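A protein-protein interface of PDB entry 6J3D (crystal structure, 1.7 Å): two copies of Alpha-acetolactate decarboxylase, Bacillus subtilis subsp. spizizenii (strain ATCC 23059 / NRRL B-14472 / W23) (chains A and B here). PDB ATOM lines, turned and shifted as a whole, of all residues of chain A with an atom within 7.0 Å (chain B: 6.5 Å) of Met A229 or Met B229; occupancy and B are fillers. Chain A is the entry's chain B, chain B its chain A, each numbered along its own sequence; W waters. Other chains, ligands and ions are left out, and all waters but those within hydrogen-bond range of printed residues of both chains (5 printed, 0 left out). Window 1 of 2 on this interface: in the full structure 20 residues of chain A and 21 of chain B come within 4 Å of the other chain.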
ATOM      1  N   SER A  26      17.999 -14.101 -31.463  1.00  0.00           N
ATOM      2  CA  SER A  26      16.949 -14.224 -32.534  1.00  0.00           C
ATOM      3  C   SER A  26      15.783 -15.052 -32.024  1.00  0.00           C
ATOM      4  O   SER A  26      15.432 -16.066 -32.615  1.00  0.00           O
ATOM      5  CB  SER A  26      17.447 -14.895 -33.822  1.00  0.00           C
ATOM      6  N   GLN A  27      15.164 -14.617 -30.945  1.00  0.00           N
ATOM      7  CA  GLN A  27      14.070 -15.400 -30.401  1.00  0.00           C
ATOM      8  C   GLN A  27      12.840 -14.563 -30.118  1.00  0.00           C
ATOM      9  O   GLN A  27      12.944 -13.389 -29.834  1.00  0.00           O
ATOM     10  CB  GLN A  27      14.481 -16.139 -29.115  1.00  0.00           C
ATOM     11  CG  GLN A  27      14.228 -15.403 -27.851  1.00  0.00           C
ATOM     12  CD  GLN A  27      14.609 -16.115 -26.566  1.00  0.00           C
ATOM     13  OE1 GLN A  27      14.968 -17.319 -26.537  1.00  0.00           O
ATOM     14  NE2 GLN A  27      14.575 -15.338 -25.479  1.00  0.00           N
ATOM     15  N   ILE A  28      11.694 -15.207 -30.205  1.00  0.00           N
ATOM     16  CA  ILE A  28      10.448 -14.701 -29.631  1.00  0.00           C
ATOM     17  C   ILE A  28      10.319 -15.343 -28.263  1.00  0.00           C
ATOM     18  O   ILE A  28      10.438 -16.576 -28.164  1.00  0.00           O
ATOM     19  CB  ILE A  28       9.277 -15.024 -30.500  1.00  0.00           C
ATOM     20  CG1 ILE A  28       9.381 -14.138 -31.780  1.00  0.00           C
ATOM     21  CG2 ILE A  28       7.928 -14.649 -29.801  1.00  0.00           C
ATOM     22  CD1 ILE A  28       8.486 -14.547 -32.813  1.00  0.00           C
ATOM     23  N   TYR A  29      10.148 -14.533 -27.226  1.00  0.00           N
ATOM     24  CA  TYR A  29       9.903 -15.016 -25.866  1.00  0.00           C
ATOM     25  C   TYR A  29       8.381 -15.059 -25.645  1.00  0.00           C
ATOM     26  O   TYR A  29       7.725 -14.033 -25.745  1.00  0.00           O
ATOM     27  CB  TYR A  29      10.625 -14.103 -24.879  1.00  0.00           C
ATOM     28  CG  TYR A  29      10.735 -14.709 -23.504  1.00  0.00           C
ATOM     29  CD1 TYR A  29      11.654 -15.706 -23.250  1.00  0.00           C
ATOM     30  CD2 TYR A  29       9.927 -14.293 -22.466  1.00  0.00           C
ATOM     31  CE1 TYR A  29      11.720 -16.276 -22.028  1.00  0.00           C
ATOM     32  CE2 TYR A  29      10.012 -14.874 -21.214  1.00  0.00           C
ATOM     33  CZ  TYR A  29      10.886 -15.861 -21.003  1.00  0.00           C
ATOM     34  OH  TYR A  29      11.021 -16.441 -19.757  1.00  0.00           O
ATOM     35  N   GLN A  30       7.808 -16.263 -25.448  1.00  0.00           N
ATOM     36  CA  GLN A  30       6.369 -16.447 -25.342  1.00  0.00           C
ATOM     37  C   GLN A  30       6.031 -16.799 -23.902  1.00  0.00           C
ATOM     38  O   GLN A  30       6.469 -17.845 -23.380  1.00  0.00           O
ATOM     39  CB  GLN A  30       5.921 -17.574 -26.277  1.00  0.00           C
ATOM     40  CG  GLN A  30       4.496 -17.986 -26.186  1.00  0.00           C
ATOM     41  CD  GLN A  30       3.590 -16.818 -26.492  1.00  0.00           C
ATOM     42  OE1 GLN A  30       3.759 -16.158 -27.550  1.00  0.00           O
ATOM     43  NE2 GLN A  30       2.651 -16.513 -25.598  1.00  0.00           N
ATOM     44  N   PHE A 133       8.799 -17.487 -37.615  1.00  0.00           N
ATOM     45  CA  PHE A 133       8.139 -16.464 -36.834  1.00  0.00           C
ATOM     46  C   PHE A 133       8.594 -15.098 -37.340  1.00  0.00           C
ATOM     47  O   PHE A 133       9.758 -14.930 -37.716  1.00  0.00           O
ATOM     48  CB  PHE A 133       8.476 -16.571 -35.349  1.00  0.00           C
ATOM     49  CG  PHE A 133       7.965 -17.807 -34.698  1.00  0.00           C
ATOM     50  CD1 PHE A 133       8.630 -18.990 -34.850  1.00  0.00           C
ATOM     51  CD2 PHE A 133       6.801 -17.744 -33.940  1.00  0.00           C
ATOM     52  CE1 PHE A 133       8.150 -20.168 -34.237  1.00  0.00           C
ATOM     53  CE2 PHE A 133       6.301 -18.885 -33.334  1.00  0.00           C
ATOM     54  CZ  PHE A 133       6.980 -20.100 -33.492  1.00  0.00           C
ATOM     55  N   TYR A 187       1.685 -24.224 -36.985  1.00  0.00           N
ATOM     56  CA  TYR A 187       2.092 -25.269 -36.034  1.00  0.00           C
ATOM     57  C   TYR A 187       2.191 -24.797 -34.578  1.00  0.00           C
ATOM     58  O   TYR A 187       2.215 -25.620 -33.632  1.00  0.00           O
ATOM     59  CB  TYR A 187       3.400 -25.972 -36.470  1.00  0.00           C
ATOM     60  CG  TYR A 187       4.632 -25.086 -36.553  1.00  0.00           C
ATOM     61  CD1 TYR A 187       5.262 -24.609 -35.417  1.00  0.00           C
ATOM     62  CD2 TYR A 187       5.192 -24.776 -37.803  1.00  0.00           C
ATOM     63  CE1 TYR A 187       6.371 -23.776 -35.495  1.00  0.00           C
ATOM     64  CE2 TYR A 187       6.330 -23.989 -37.890  1.00  0.00           C
ATOM     65  CZ  TYR A 187       6.907 -23.483 -36.737  1.00  0.00           C
ATOM     66  OH  TYR A 187       8.033 -22.668 -36.823  1.00  0.00           O
ATOM     67  N   ALA A 188       2.213 -23.480 -34.389  1.00  0.00           N
ATOM     68  CA  ALA A 188       2.252 -22.887 -33.071  1.00  0.00           C
ATOM     69  C   ALA A 188       0.909 -22.376 -32.617  1.00  0.00           C
ATOM     70  O   ALA A 188       0.848 -21.746 -31.573  1.00  0.00           O
ATOM     71  CB  ALA A 188       3.301 -21.780 -33.000  1.00  0.00           C
ATOM     72  N   ILE A 191      -0.437 -22.288 -28.787  1.00  0.00           N
ATOM     73  CA  ILE A 191       0.603 -21.598 -28.016  1.00  0.00           C
ATOM     74  C   ILE A 191       0.482 -20.091 -28.189  1.00  0.00           C
ATOM     75  O   ILE A 191       0.338 -19.355 -27.202  1.00  0.00           O
ATOM     76  CB  ILE A 191       2.029 -22.106 -28.359  1.00  0.00           C
ATOM     77  CG1 ILE A 191       2.193 -23.548 -27.914  1.00  0.00           C
ATOM     78  CG2 ILE A 191       3.092 -21.255 -27.703  1.00  0.00           C
ATOM     79  CD1 ILE A 191       3.530 -24.199 -28.365  1.00  0.00           C
ATOM     80  N   ALA A 192       0.509 -19.632 -29.433  1.00  0.00           N
ATOM     81  CA  ALA A 192       0.300 -18.228 -29.758  1.00  0.00           C
ATOM     82  C   ALA A 192      -0.875 -18.168 -30.731  1.00  0.00           C
ATOM     83  O   ALA A 192      -1.571 -19.159 -30.942  1.00  0.00           O
ATOM     84  CB  ALA A 192       1.563 -17.560 -30.298  1.00  0.00           C
ATOM     85  N   LYS A 226      12.440 -14.258 -37.080  1.00  0.00           N
ATOM     86  CA  LYS A 226      12.940 -14.910 -35.888  1.00  0.00           C
ATOM     87  C   LYS A 226      12.913 -16.419 -36.054  1.00  0.00           C
ATOM     88  O   LYS A 226      11.907 -16.980 -36.474  1.00  0.00           O
ATOM     89  CB  LYS A 226      12.146 -14.512 -34.663  1.00  0.00           C
ATOM     90  CG  LYS A 226      12.126 -13.019 -34.380  1.00  0.00           C
ATOM     91  CD  LYS A 226      13.475 -12.541 -33.883  1.00  0.00           C
ATOM     92  CE  LYS A 226      13.494 -11.023 -33.824  1.00  0.00           C
ATOM     93  NZ  LYS A 226      14.870 -10.517 -33.700  1.00  0.00           N
ATOM     94  N   MET A 227      14.003 -17.046 -35.625  1.00  0.00           N
ATOM     95  CA  MET A 227      14.254 -18.468 -35.824  1.00  0.00           C
ATOM     96  C   MET A 227      14.052 -19.313 -34.562  1.00  0.00           C
ATOM     97  O   MET A 227      14.260 -20.507 -34.607  1.00  0.00           O
ATOM     98  CB  MET A 227      15.716 -18.634 -36.251  1.00  0.00           C
ATOM     99  CG  MET A 227      16.079 -17.904 -37.535  1.00  0.00           C
ATOM    100  SD  MET A 227      14.981 -18.439 -38.839  1.00  0.00           S
ATOM    101  CE  MET A 227      15.745 -19.984 -39.363  1.00  0.00           C
ATOM    102  N   ASN A 228      13.714 -18.703 -33.445  1.00  0.00           N
ATOM    103  CA  ASN A 228      13.570 -19.423 -32.186  1.00  0.00           C
ATOM    104  C   ASN A 228      12.376 -18.887 -31.474  1.00  0.00           C
ATOM    105  O   ASN A 228      12.078 -17.718 -31.535  1.00  0.00           O
ATOM    106  CB  ASN A 228      14.835 -19.295 -31.303  1.00  0.00           C
ATOM    107  CG  ASN A 228      16.135 -19.673 -32.073  1.00  0.00           C
ATOM    108  OD1 ASN A 228      16.357 -20.832 -32.356  1.00  0.00           O
ATOM    109  ND2 ASN A 228      16.958 -18.697 -32.441  1.00  0.00           N
ATOM    110  N   MET A 229      11.680 -19.777 -30.781  1.00  0.00           N
ATOM    111  CA  MET A 229      10.523 -19.429 -29.953  1.00  0.00           C
ATOM    112  C   MET A 229      10.699 -20.098 -28.600  1.00  0.00           C
ATOM    113  O   MET A 229      10.739 -21.336 -28.540  1.00  0.00           O
ATOM    114  CB  MET A 229       9.236 -19.940 -30.624  1.00  0.00           C
ATOM    115  CG  MET A 229       7.964 -19.442 -29.987  1.00  0.00           C
ATOM    116  SD  MET A 229       7.646 -20.266 -28.432  1.00  0.00           S
ATOM    117  CE  MET A 229       7.126 -21.871 -29.020  1.00  0.00           C
ATOM    118  N   ASN A 230      10.795 -19.314 -27.521  1.00  0.00           N
ATOM    119  CA  ASN A 230      10.907 -19.899 -26.159  1.00  0.00           C
ATOM    120  C   ASN A 230       9.654 -19.701 -25.387  1.00  0.00           C
ATOM    121  O   ASN A 230       9.272 -18.560 -25.150  1.00  0.00           O
ATOM    122  CB  ASN A 230      12.067 -19.351 -25.344  1.00  0.00           C
ATOM    123  CG  ASN A 230      12.127 -20.027 -23.951  1.00  0.00           C
ATOM    124  OD1 ASN A 230      12.679 -21.052 -23.818  1.00  0.00           O
ATOM    125  ND2 ASN A 230      11.346 -19.517 -22.980  1.00  0.00           N
ATOM    126  N   LEU A 231       8.991 -20.811 -25.035  1.00  0.00           N
ATOM    127  CA  LEU A 231       7.774 -20.800 -24.296  1.00  0.00           C
ATOM    128  C   LEU A 231       8.083 -20.968 -22.834  1.00  0.00           C
ATOM    129  O   LEU A 231       8.722 -21.972 -22.450  1.00  0.00           O
ATOM    130  CB  LEU A 231       6.886 -21.944 -24.762  1.00  0.00           C
ATOM    131  CG  LEU A 231       5.617 -22.203 -23.979  1.00  0.00           C
ATOM    132  CD1 LEU A 231       4.678 -20.978 -23.950  1.00  0.00           C
ATOM    133  CD2 LEU A 231       4.895 -23.499 -24.490  1.00  0.00           C
ATOM    134  N   ARG A 232       7.611 -20.007 -22.025  1.00  0.00           N
ATOM    135  CA  ARG A 232       7.793 -20.014 -20.591  1.00  0.00           C
ATOM    136  C   ARG A 232       6.445 -20.281 -19.950  1.00  0.00           C
ATOM    137  O   ARG A 232       5.480 -19.540 -20.169  1.00  0.00           O
ATOM    138  CB  ARG A 232       8.249 -18.639 -20.162  1.00  0.00           C
ATOM    139  CG  ARG A 232       8.432 -18.507 -18.692  1.00  0.00           C
ATOM    140  CD  ARG A 232       8.182 -17.099 -18.287  1.00  0.00           C
ATOM    141  NE  ARG A 232       8.361 -16.963 -16.846  1.00  0.00           N
ATOM    142  CZ  ARG A 232       9.421 -16.434 -16.250  1.00  0.00           C
ATOM    143  NH1 ARG A 232      10.465 -15.981 -16.956  1.00  0.00           N
ATOM    144  NH2 ARG A 232       9.423 -16.360 -14.921  1.00  0.00           N
ATOM    145  N   LEU A 233       6.359 -21.336 -19.163  1.00  0.00           N
ATOM    146  CA  LEU A 233       5.110 -21.687 -18.483  1.00  0.00           C
ATOM    147  C   LEU A 233       5.045 -21.095 -17.088  1.00  0.00           C
ATOM    148  O   LEU A 233       6.051 -20.961 -16.405  1.00  0.00           O
ATOM    149  CB  LEU A 233       4.954 -23.220 -18.381  1.00  0.00           C
ATOM    150  CG  LEU A 233       5.038 -23.931 -19.757  1.00  0.00           C
ATOM    151  CD1 LEU A 233       5.006 -25.463 -19.528  1.00  0.00           C
ATOM    152  CD2 LEU A 233       3.946 -23.397 -20.779  1.00  0.00           C
ATOM    153  N   SER B  26      15.602 -24.746 -16.543  1.00  0.00           N
ATOM    154  CA  SER B  26      14.415 -25.630 -16.610  1.00  0.00           C
ATOM    155  C   SER B  26      13.861 -25.571 -18.024  1.00  0.00           C
ATOM    156  O   SER B  26      12.770 -25.065 -18.243  1.00  0.00           O
ATOM    157  CB  SER B  26      13.338 -25.169 -15.599  1.00  0.00           C
ATOM    158  OG  SER B  26      12.234 -26.086 -15.481  1.00  0.00           O
ATOM    159  N   GLN B  27      14.603 -26.056 -19.004  1.00  0.00           N
ATOM    160  CA  GLN B  27      14.090 -26.038 -20.361  1.00  0.00           C
ATOM    161  C   GLN B  27      14.274 -27.347 -21.097  1.00  0.00           C
ATOM    162  O   GLN B  27      15.240 -28.086 -20.822  1.00  0.00           O
ATOM    163  CB  GLN B  27      14.748 -24.915 -21.171  1.00  0.00           C
ATOM    164  CG  GLN B  27      16.114 -25.180 -21.618  1.00  0.00           C
ATOM    165  CD  GLN B  27      16.625 -24.185 -22.607  1.00  0.00           C
ATOM    166  OE1 GLN B  27      16.013 -23.126 -22.855  1.00  0.00           O
ATOM    167  NE2 GLN B  27      17.792 -24.511 -23.186  1.00  0.00           N
ATOM    168  N   ILE B  28      13.351 -27.631 -22.021  1.00  0.00           N
ATOM    169  CA  ILE B  28      13.561 -28.597 -23.091  1.00  0.00           C
ATOM    170  C   ILE B  28      14.014 -27.822 -24.321  1.00  0.00           C
ATOM    171  O   ILE B  28      13.415 -26.811 -24.652  1.00  0.00           O
ATOM    172  CB  ILE B  28      12.296 -29.391 -23.391  1.00  0.00           C
ATOM    173  CG1 ILE B  28      11.903 -30.249 -22.168  1.00  0.00           C
ATOM    174  CG2 ILE B  28      12.427 -30.255 -24.639  1.00  0.00           C
ATOM    175  CD1 ILE B  28      10.690 -30.947 -22.419  1.00  0.00           C
ATOM    176  N   TYR B  29      15.129 -28.242 -24.935  1.00  0.00           N
ATOM    177  CA  TYR B  29      15.638 -27.638 -26.106  1.00  0.00           C
ATOM    178  C   TYR B  29      15.190 -28.503 -27.255  1.00  0.00           C
ATOM    179  O   TYR B  29      15.601 -29.677 -27.363  1.00  0.00           O
ATOM    180  CB  TYR B  29      17.158 -27.503 -26.037  1.00  0.00           C
ATOM    181  CG  TYR B  29      17.726 -26.608 -27.068  1.00  0.00           C
ATOM    182  CD1 TYR B  29      17.676 -25.228 -26.903  1.00  0.00           C
ATOM    183  CD2 TYR B  29      18.342 -27.125 -28.198  1.00  0.00           C
ATOM    184  CE1 TYR B  29      18.203 -24.378 -27.852  1.00  0.00           C
ATOM    185  CE2 TYR B  29      18.882 -26.273 -29.166  1.00  0.00           C
ATOM    186  CZ  TYR B  29      18.797 -24.903 -28.967  1.00  0.00           C
ATOM    187  OH  TYR B  29      19.284 -23.998 -29.876  1.00  0.00           O
ATOM    188  N   GLN B  30      14.324 -27.916 -28.089  1.00  0.00           N
ATOM    189  CA  GLN B  30      13.612 -28.589 -29.165  1.00  0.00           C
ATOM    190  C   GLN B  30      14.131 -28.162 -30.518  1.00  0.00           C
ATOM    191  O   GLN B  30      14.002 -27.015 -30.902  1.00  0.00           O
ATOM    192  CB  GLN B  30      12.113 -28.316 -29.085  1.00  0.00           C
ATOM    193  CG  GLN B  30      11.294 -28.943 -30.218  1.00  0.00           C
ATOM    194  CD  GLN B  30      11.444 -30.432 -30.245  1.00  0.00           C
ATOM    195  OE1 GLN B  30      11.318 -31.082 -29.164  1.00  0.00           O
ATOM    196  NE2 GLN B  30      11.776 -31.011 -31.428  1.00  0.00           N
ATOM    197  N   PHE B 133       5.954 -29.740 -19.325  1.00  0.00           N
ATOM    198  CA  PHE B 133       6.854 -30.667 -20.024  1.00  0.00           C
ATOM    199  C   PHE B 133       7.605 -31.491 -18.985  1.00  0.00           C
ATOM    200  O   PHE B 133       7.931 -31.007 -17.903  1.00  0.00           O
ATOM    201  CB  PHE B 133       7.844 -29.899 -20.858  1.00  0.00           C
ATOM    202  CG  PHE B 133       7.231 -29.187 -22.042  1.00  0.00           C
ATOM    203  CD1 PHE B 133       6.674 -27.945 -21.885  1.00  0.00           C
ATOM    204  CD2 PHE B 133       7.249 -29.771 -23.309  1.00  0.00           C
ATOM    205  CE1 PHE B 133       6.100 -27.311 -22.980  1.00  0.00           C
ATOM    206  CE2 PHE B 133       6.719 -29.118 -24.396  1.00  0.00           C
ATOM    207  CZ  PHE B 133       6.120 -27.905 -24.218  1.00  0.00           C
ATOM    208  N   THR B 184       5.025 -34.583 -23.418  1.00  0.00           N
ATOM    209  CA  THR B 184       4.708 -33.318 -24.079  1.00  0.00           C
ATOM    210  C   THR B 184       3.218 -33.051 -23.981  1.00  0.00           C
ATOM    211  O   THR B 184       2.382 -33.913 -24.316  1.00  0.00           O
ATOM    212  CB  THR B 184       5.115 -33.378 -25.544  1.00  0.00           C
ATOM    213  OG1 THR B 184       6.547 -33.537 -25.617  1.00  0.00           O
ATOM    214  CG2 THR B 184       4.743 -32.134 -26.264  1.00  0.00           C
ATOM    215  N   ALA B 188       1.428 -28.621 -27.687  1.00  0.00           N
ATOM    216  CA  ALA B 188       2.700 -28.627 -28.402  1.00  0.00           C
ATOM    217  C   ALA B 188       2.749 -29.719 -29.482  1.00  0.00           C
ATOM    218  O   ALA B 188       3.803 -29.959 -30.022  1.00  0.00           O
ATOM    219  CB  ALA B 188       3.872 -28.751 -27.428  1.00  0.00           C
ATOM    220  N   ILE B 191       4.764 -29.544 -32.948  1.00  0.00           N
ATOM    221  CA  ILE B 191       6.156 -29.165 -32.653  1.00  0.00           C
ATOM    222  C   ILE B 191       6.926 -30.399 -32.157  1.00  0.00           C
ATOM    223  O   ILE B 191       7.979 -30.825 -32.715  1.00  0.00           O
ATOM    224  CB  ILE B 191       6.237 -27.985 -31.646  1.00  0.00           C
ATOM    225  CG1 ILE B 191       5.627 -26.738 -32.289  1.00  0.00           C
ATOM    226  CG2 ILE B 191       7.685 -27.812 -31.189  1.00  0.00           C
ATOM    227  CD1 ILE B 191       5.224 -25.659 -31.296  1.00  0.00           C
ATOM    228  N   ALA B 192       6.433 -30.985 -31.061  1.00  0.00           N
ATOM    229  CA  ALA B 192       6.979 -32.244 -30.554  1.00  0.00           C
ATOM    230  C   ALA B 192       5.885 -33.301 -30.657  1.00  0.00           C
ATOM    231  O   ALA B 192       4.845 -33.074 -31.260  1.00  0.00           O
ATOM    232  CB  ALA B 192       7.493 -32.087 -29.101  1.00  0.00           C
ATOM    233  N   LYS B 226       9.897 -29.619 -16.464  1.00  0.00           N
ATOM    234  CA  LYS B 226      10.493 -28.533 -17.245  1.00  0.00           C
ATOM    235  C   LYS B 226       9.475 -27.452 -17.517  1.00  0.00           C
ATOM    236  O   LYS B 226       8.367 -27.791 -17.945  1.00  0.00           O
ATOM    237  CB  LYS B 226      11.046 -29.050 -18.553  1.00  0.00           C
ATOM    238  CG  LYS B 226      12.191 -30.109 -18.346  1.00  0.00           C
ATOM    239  CD  LYS B 226      13.357 -29.536 -17.593  1.00  0.00           C
ATOM    240  CE  LYS B 226      14.351 -30.642 -17.161  1.00  0.00           C
ATOM    241  NZ  LYS B 226      15.455 -30.128 -16.312  1.00  0.00           N
ATOM    242  N   MET B 227       9.856 -26.194 -17.266  1.00  0.00           N
ATOM    243  CA  MET B 227       8.888 -25.073 -17.312  1.00  0.00           C
ATOM    244  C   MET B 227       9.068 -24.241 -18.590  1.00  0.00           C
ATOM    245  O   MET B 227       8.352 -23.264 -18.802  1.00  0.00           O
ATOM    246  CB  MET B 227       9.088 -24.151 -16.110  1.00  0.00           C
ATOM    247  CG  MET B 227       8.857 -24.805 -14.778  1.00  0.00           C
ATOM    248  SD  MET B 227       7.193 -25.510 -14.674  1.00  0.00           S
ATOM    249  CE  MET B 227       6.212 -24.084 -14.281  1.00  0.00           C
ATOM    250  N   ASN B 228      10.032 -24.598 -19.428  1.00  0.00           N
ATOM    251  CA  ASN B 228      10.276 -23.875 -20.662  1.00  0.00           C
ATOM    252  C   ASN B 228      10.509 -24.845 -21.800  1.00  0.00           C
ATOM    253  O   ASN B 228      11.115 -25.907 -21.612  1.00  0.00           O
ATOM    254  CB  ASN B 228      11.538 -23.030 -20.582  1.00  0.00           C
ATOM    255  CG  ASN B 228      11.403 -21.876 -19.704  1.00  0.00           C
ATOM    256  OD1 ASN B 228      11.033 -20.746 -20.167  1.00  0.00           O
ATOM    257  ND2 ASN B 228      11.794 -22.068 -18.446  1.00  0.00           N
ATOM    258  N   MET B 229      10.056 -24.488 -22.988  1.00  0.00           N
ATOM    259  CA  MET B 229      10.389 -25.204 -24.187  1.00  0.00           C
ATOM    260  C   MET B 229      10.923 -24.219 -25.212  1.00  0.00           C
ATOM    261  O   MET B 229      10.195 -23.310 -25.612  1.00  0.00           O
ATOM    262  CB  MET B 229       9.150 -25.843 -24.757  1.00  0.00           C
ATOM    263  CG  MET B 229       9.550 -26.895 -25.612  1.00  0.00           C
ATOM    264  SD  MET B 229       9.556 -26.353 -27.228  1.00  0.00           S
ATOM    265  CE  MET B 229       7.979 -27.215 -27.461  1.00  0.00           C
ATOM    266  N   ASN B 230      12.172 -24.411 -25.631  1.00  0.00           N
ATOM    267  CA  ASN B 230      12.875 -23.481 -26.528  1.00  0.00           C
ATOM    268  C   ASN B 230      12.945 -24.159 -27.885  1.00  0.00           C
ATOM    269  O   ASN B 230      13.697 -25.135 -28.043  1.00  0.00           O
ATOM    270  CB  ASN B 230      14.240 -23.310 -25.888  1.00  0.00           C
ATOM    271  CG  ASN B 230      15.017 -22.229 -26.425  1.00  0.00           C
ATOM    272  OD1 ASN B 230      14.729 -21.676 -27.502  1.00  0.00           O
ATOM    273  ND2 ASN B 230      16.098 -21.887 -25.662  1.00  0.00           N
ATOM    274  N   LEU B 231      12.182 -23.670 -28.856  1.00  0.00           N
ATOM    275  CA  LEU B 231      12.140 -24.238 -30.199  1.00  0.00           C
ATOM    276  C   LEU B 231      13.137 -23.531 -31.101  1.00  0.00           C
ATOM    277  O   LEU B 231      13.086 -22.310 -31.228  1.00  0.00           O
ATOM    278  CB  LEU B 231      10.758 -24.082 -30.779  1.00  0.00           C
ATOM    279  CG  LEU B 231      10.535 -24.400 -32.249  1.00  0.00           C
ATOM    280  CD1 LEU B 231      10.846 -25.879 -32.549  1.00  0.00           C
ATOM    281  CD2 LEU B 231       9.091 -24.060 -32.642  1.00  0.00           C
ATOM    282  N   ARG B 232      13.997 -24.322 -31.732  1.00  0.00           N
ATOM    283  CA  ARG B 232      15.070 -23.831 -32.597  1.00  0.00           C
ATOM    284  C   ARG B 232      14.728 -24.283 -34.006  1.00  0.00           C
ATOM    285  O   ARG B 232      14.722 -25.489 -34.279  1.00  0.00           O
ATOM    286  CB  ARG B 232      16.400 -24.417 -32.117  1.00  0.00           C
ATOM    287  CG  ARG B 232      17.577 -24.041 -33.011  1.00  0.00           C
ATOM    288  CD  ARG B 232      18.696 -25.028 -32.981  1.00  0.00           C
ATOM    289  NE  ARG B 232      19.854 -24.605 -33.802  1.00  0.00           N
ATOM    290  CZ  ARG B 232      21.037 -24.202 -33.320  1.00  0.00           C
ATOM    291  NH1 ARG B 232      21.274 -24.114 -32.004  1.00  0.00           N
ATOM    292  NH2 ARG B 232      22.008 -23.880 -34.181  1.00  0.00           N
ATOM    293  N   LEU B 233      14.519 -23.334 -34.913  1.00  0.00           N
ATOM    294  CA  LEU B 233      14.150 -23.629 -36.292  1.00  0.00           C
ATOM    295  C   LEU B 233      15.415 -23.734 -37.146  1.00  0.00           C
ATOM    296  O   LEU B 233      16.413 -23.012 -36.908  1.00  0.00           O
ATOM    297  CB  LEU B 233      13.193 -22.598 -36.874  1.00  0.00           C
ATOM    298  CG  LEU B 233      11.858 -22.516 -36.138  1.00  0.00           C
ATOM    299  CD1 LEU B 233      11.024 -21.465 -36.786  1.00  0.00           C
ATOM    300  CD2 LEU B 233      11.127 -23.869 -36.085  1.00  0.00           C
HETATM  301  O   HOH W   1      14.183 -21.489 -21.764  1.00  0.00           O
HETATM  302  O   HOH W   2      17.809 -21.355 -34.961  1.00  0.00           O
HETATM  303  O   HOH W   3      18.694 -21.645 -29.898  1.00  0.00           O
HETATM  304  O   HOH W   4      15.868 -19.315 -28.141  1.00  0.00           O
HETATM  305  O   HOH W   5      12.311 -18.516 -19.345  1.00  0.00           O
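Of the 18 printed residues of chain B, 9 touch a printed residue of chain A. Of the 18 printed residues of chain A, 10 touch a printed residue of chain B. Printed residues of chain A that touch a printed residue of chain B: Phe A133, Tyr A187, Ile A191, Met A227, Asn A228, Met A229, Asn A230, Leu A231, Arg A232 and Leu A233. Among the printed residues, no Asp or Glu carboxylate lies within 4 Å of a Lys or Arg side-chain nitrogen of the other chain.
Of the printed residues of chain B, Ile A191 touches Ile B191 (3.7 Å). Of the printed residues of chain B, Phe A133 touches Leu B233. Of the printed residues of chain B, Asn A230 touches Asn B228 (3.1 Å), Met B229 (3.5 Å) and Asn B230 (3.4 Å). Gln A27 touches none of the printed residues of chain B. Tyr B29 touches none of the printed residues of chain A.
Among the printed residues, pairs that only touch across the chains: Asn A228 with Leu B231 (3.1 Å), Tyr A187 with Leu B233 (3.2 Å), Asn A228 with Arg B232 (3.3 Å), Arg A232 with Asn B228 (3.3 Å), Asn A230 with Asn B230 (3.4 Å), Asn A230 with Met B229 (3.5 Å), Met A229 with Met B229 (3.6 Å), Met A229 with Asn B230 (3.6 Å), Ile A191 with Ile B191 (3.7 Å), Arg A232 with Met B227 (3.7 Å), Tyr A187 with Ile B191 (3.8 Å), Leu A233 with Phe B133 (3.8 Å), Met A227 with Arg B232 (3.9 Å), Leu A231 with Met B227 (3.9 Å), Phe A133 with Leu B233 (3.95 Å) and Tyr A187 with Leu B231 (3.95 Å).
The backbone carbonyl oxygen (O) of Met B229 is in hydrogen-bond range of the backbone NH (N) of Leu A231, 2.8 Å away. N of Leu B231 is in hydrogen-bond range of O of Met A229 (2.8 Å). The backbone NH (N) of Leu B233 is in hydrogen-bond range of the backbone carbonyl oxygen (O) of Met A227. The side-chain amide oxygen of Asn B228 lies close to the backbone carbonyl oxygen of Leu A231 (3.5 Å). The backbone carbonyl oxygen (O) of Met B227 is in hydrogen-bond range of the backbone NH (N) of Leu A233 (2.8 Å). The side-chain amide oxygen (OD1) of Asn B228 is in hydrogen-bond range of the side-chain amide nitrogen (ND2) of Asn A230.
Water W3 lies within hydrogen-bond range of OH of Tyr B29 (2.4 Å) and OD1 of Asn A228 (3.5 Å). Water W5 bridges OH of Tyr A29 (2.5 Å) and OD1 of Asn B228 (2.7 Å). Water W1 bridges the side-chain amide oxygen (OD1) of Asn A230 (2.6 Å) and the side-chain amide oxygen (OE1) of Gln B27 (2.7 Å). Water W2 bridges O of Leu B233 (2.9 Å) and OD1 of Asn A228 (3.0 Å).
Ile A191 touches its own counterpart, Ile B191. Met A227 touches Leu B233, and with the chains exchanged Leu A233 touches Met B227. Asn A228 touches Leu B231, and with the chains exchanged Leu A231 touches Asn B228. Met A229 touches Asn B230, and with the chains exchanged Asn A230 touches Met B229. Of the 22 pairs that touch across the chains among the printed residues, 17 have their exchanged pair printed and touching as well.
OE1 of Gln B27 is in hydrogen-bond range of ND2 of Asn B230 (3.1 Å). O of Ile B28 is in hydrogen-bond range of N of Asn B230 (2.9 Å). The backbone carbonyl oxygen (O) of Asn B230 lies within hydrogen-bond range of the backbone NH (N) of Gln B30 (2.9 Å). The backbone carbonyl oxygen of Phe A133 sits at hydrogen-bond distance from the backbone NH of Lys A226, at 2.8 Å.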
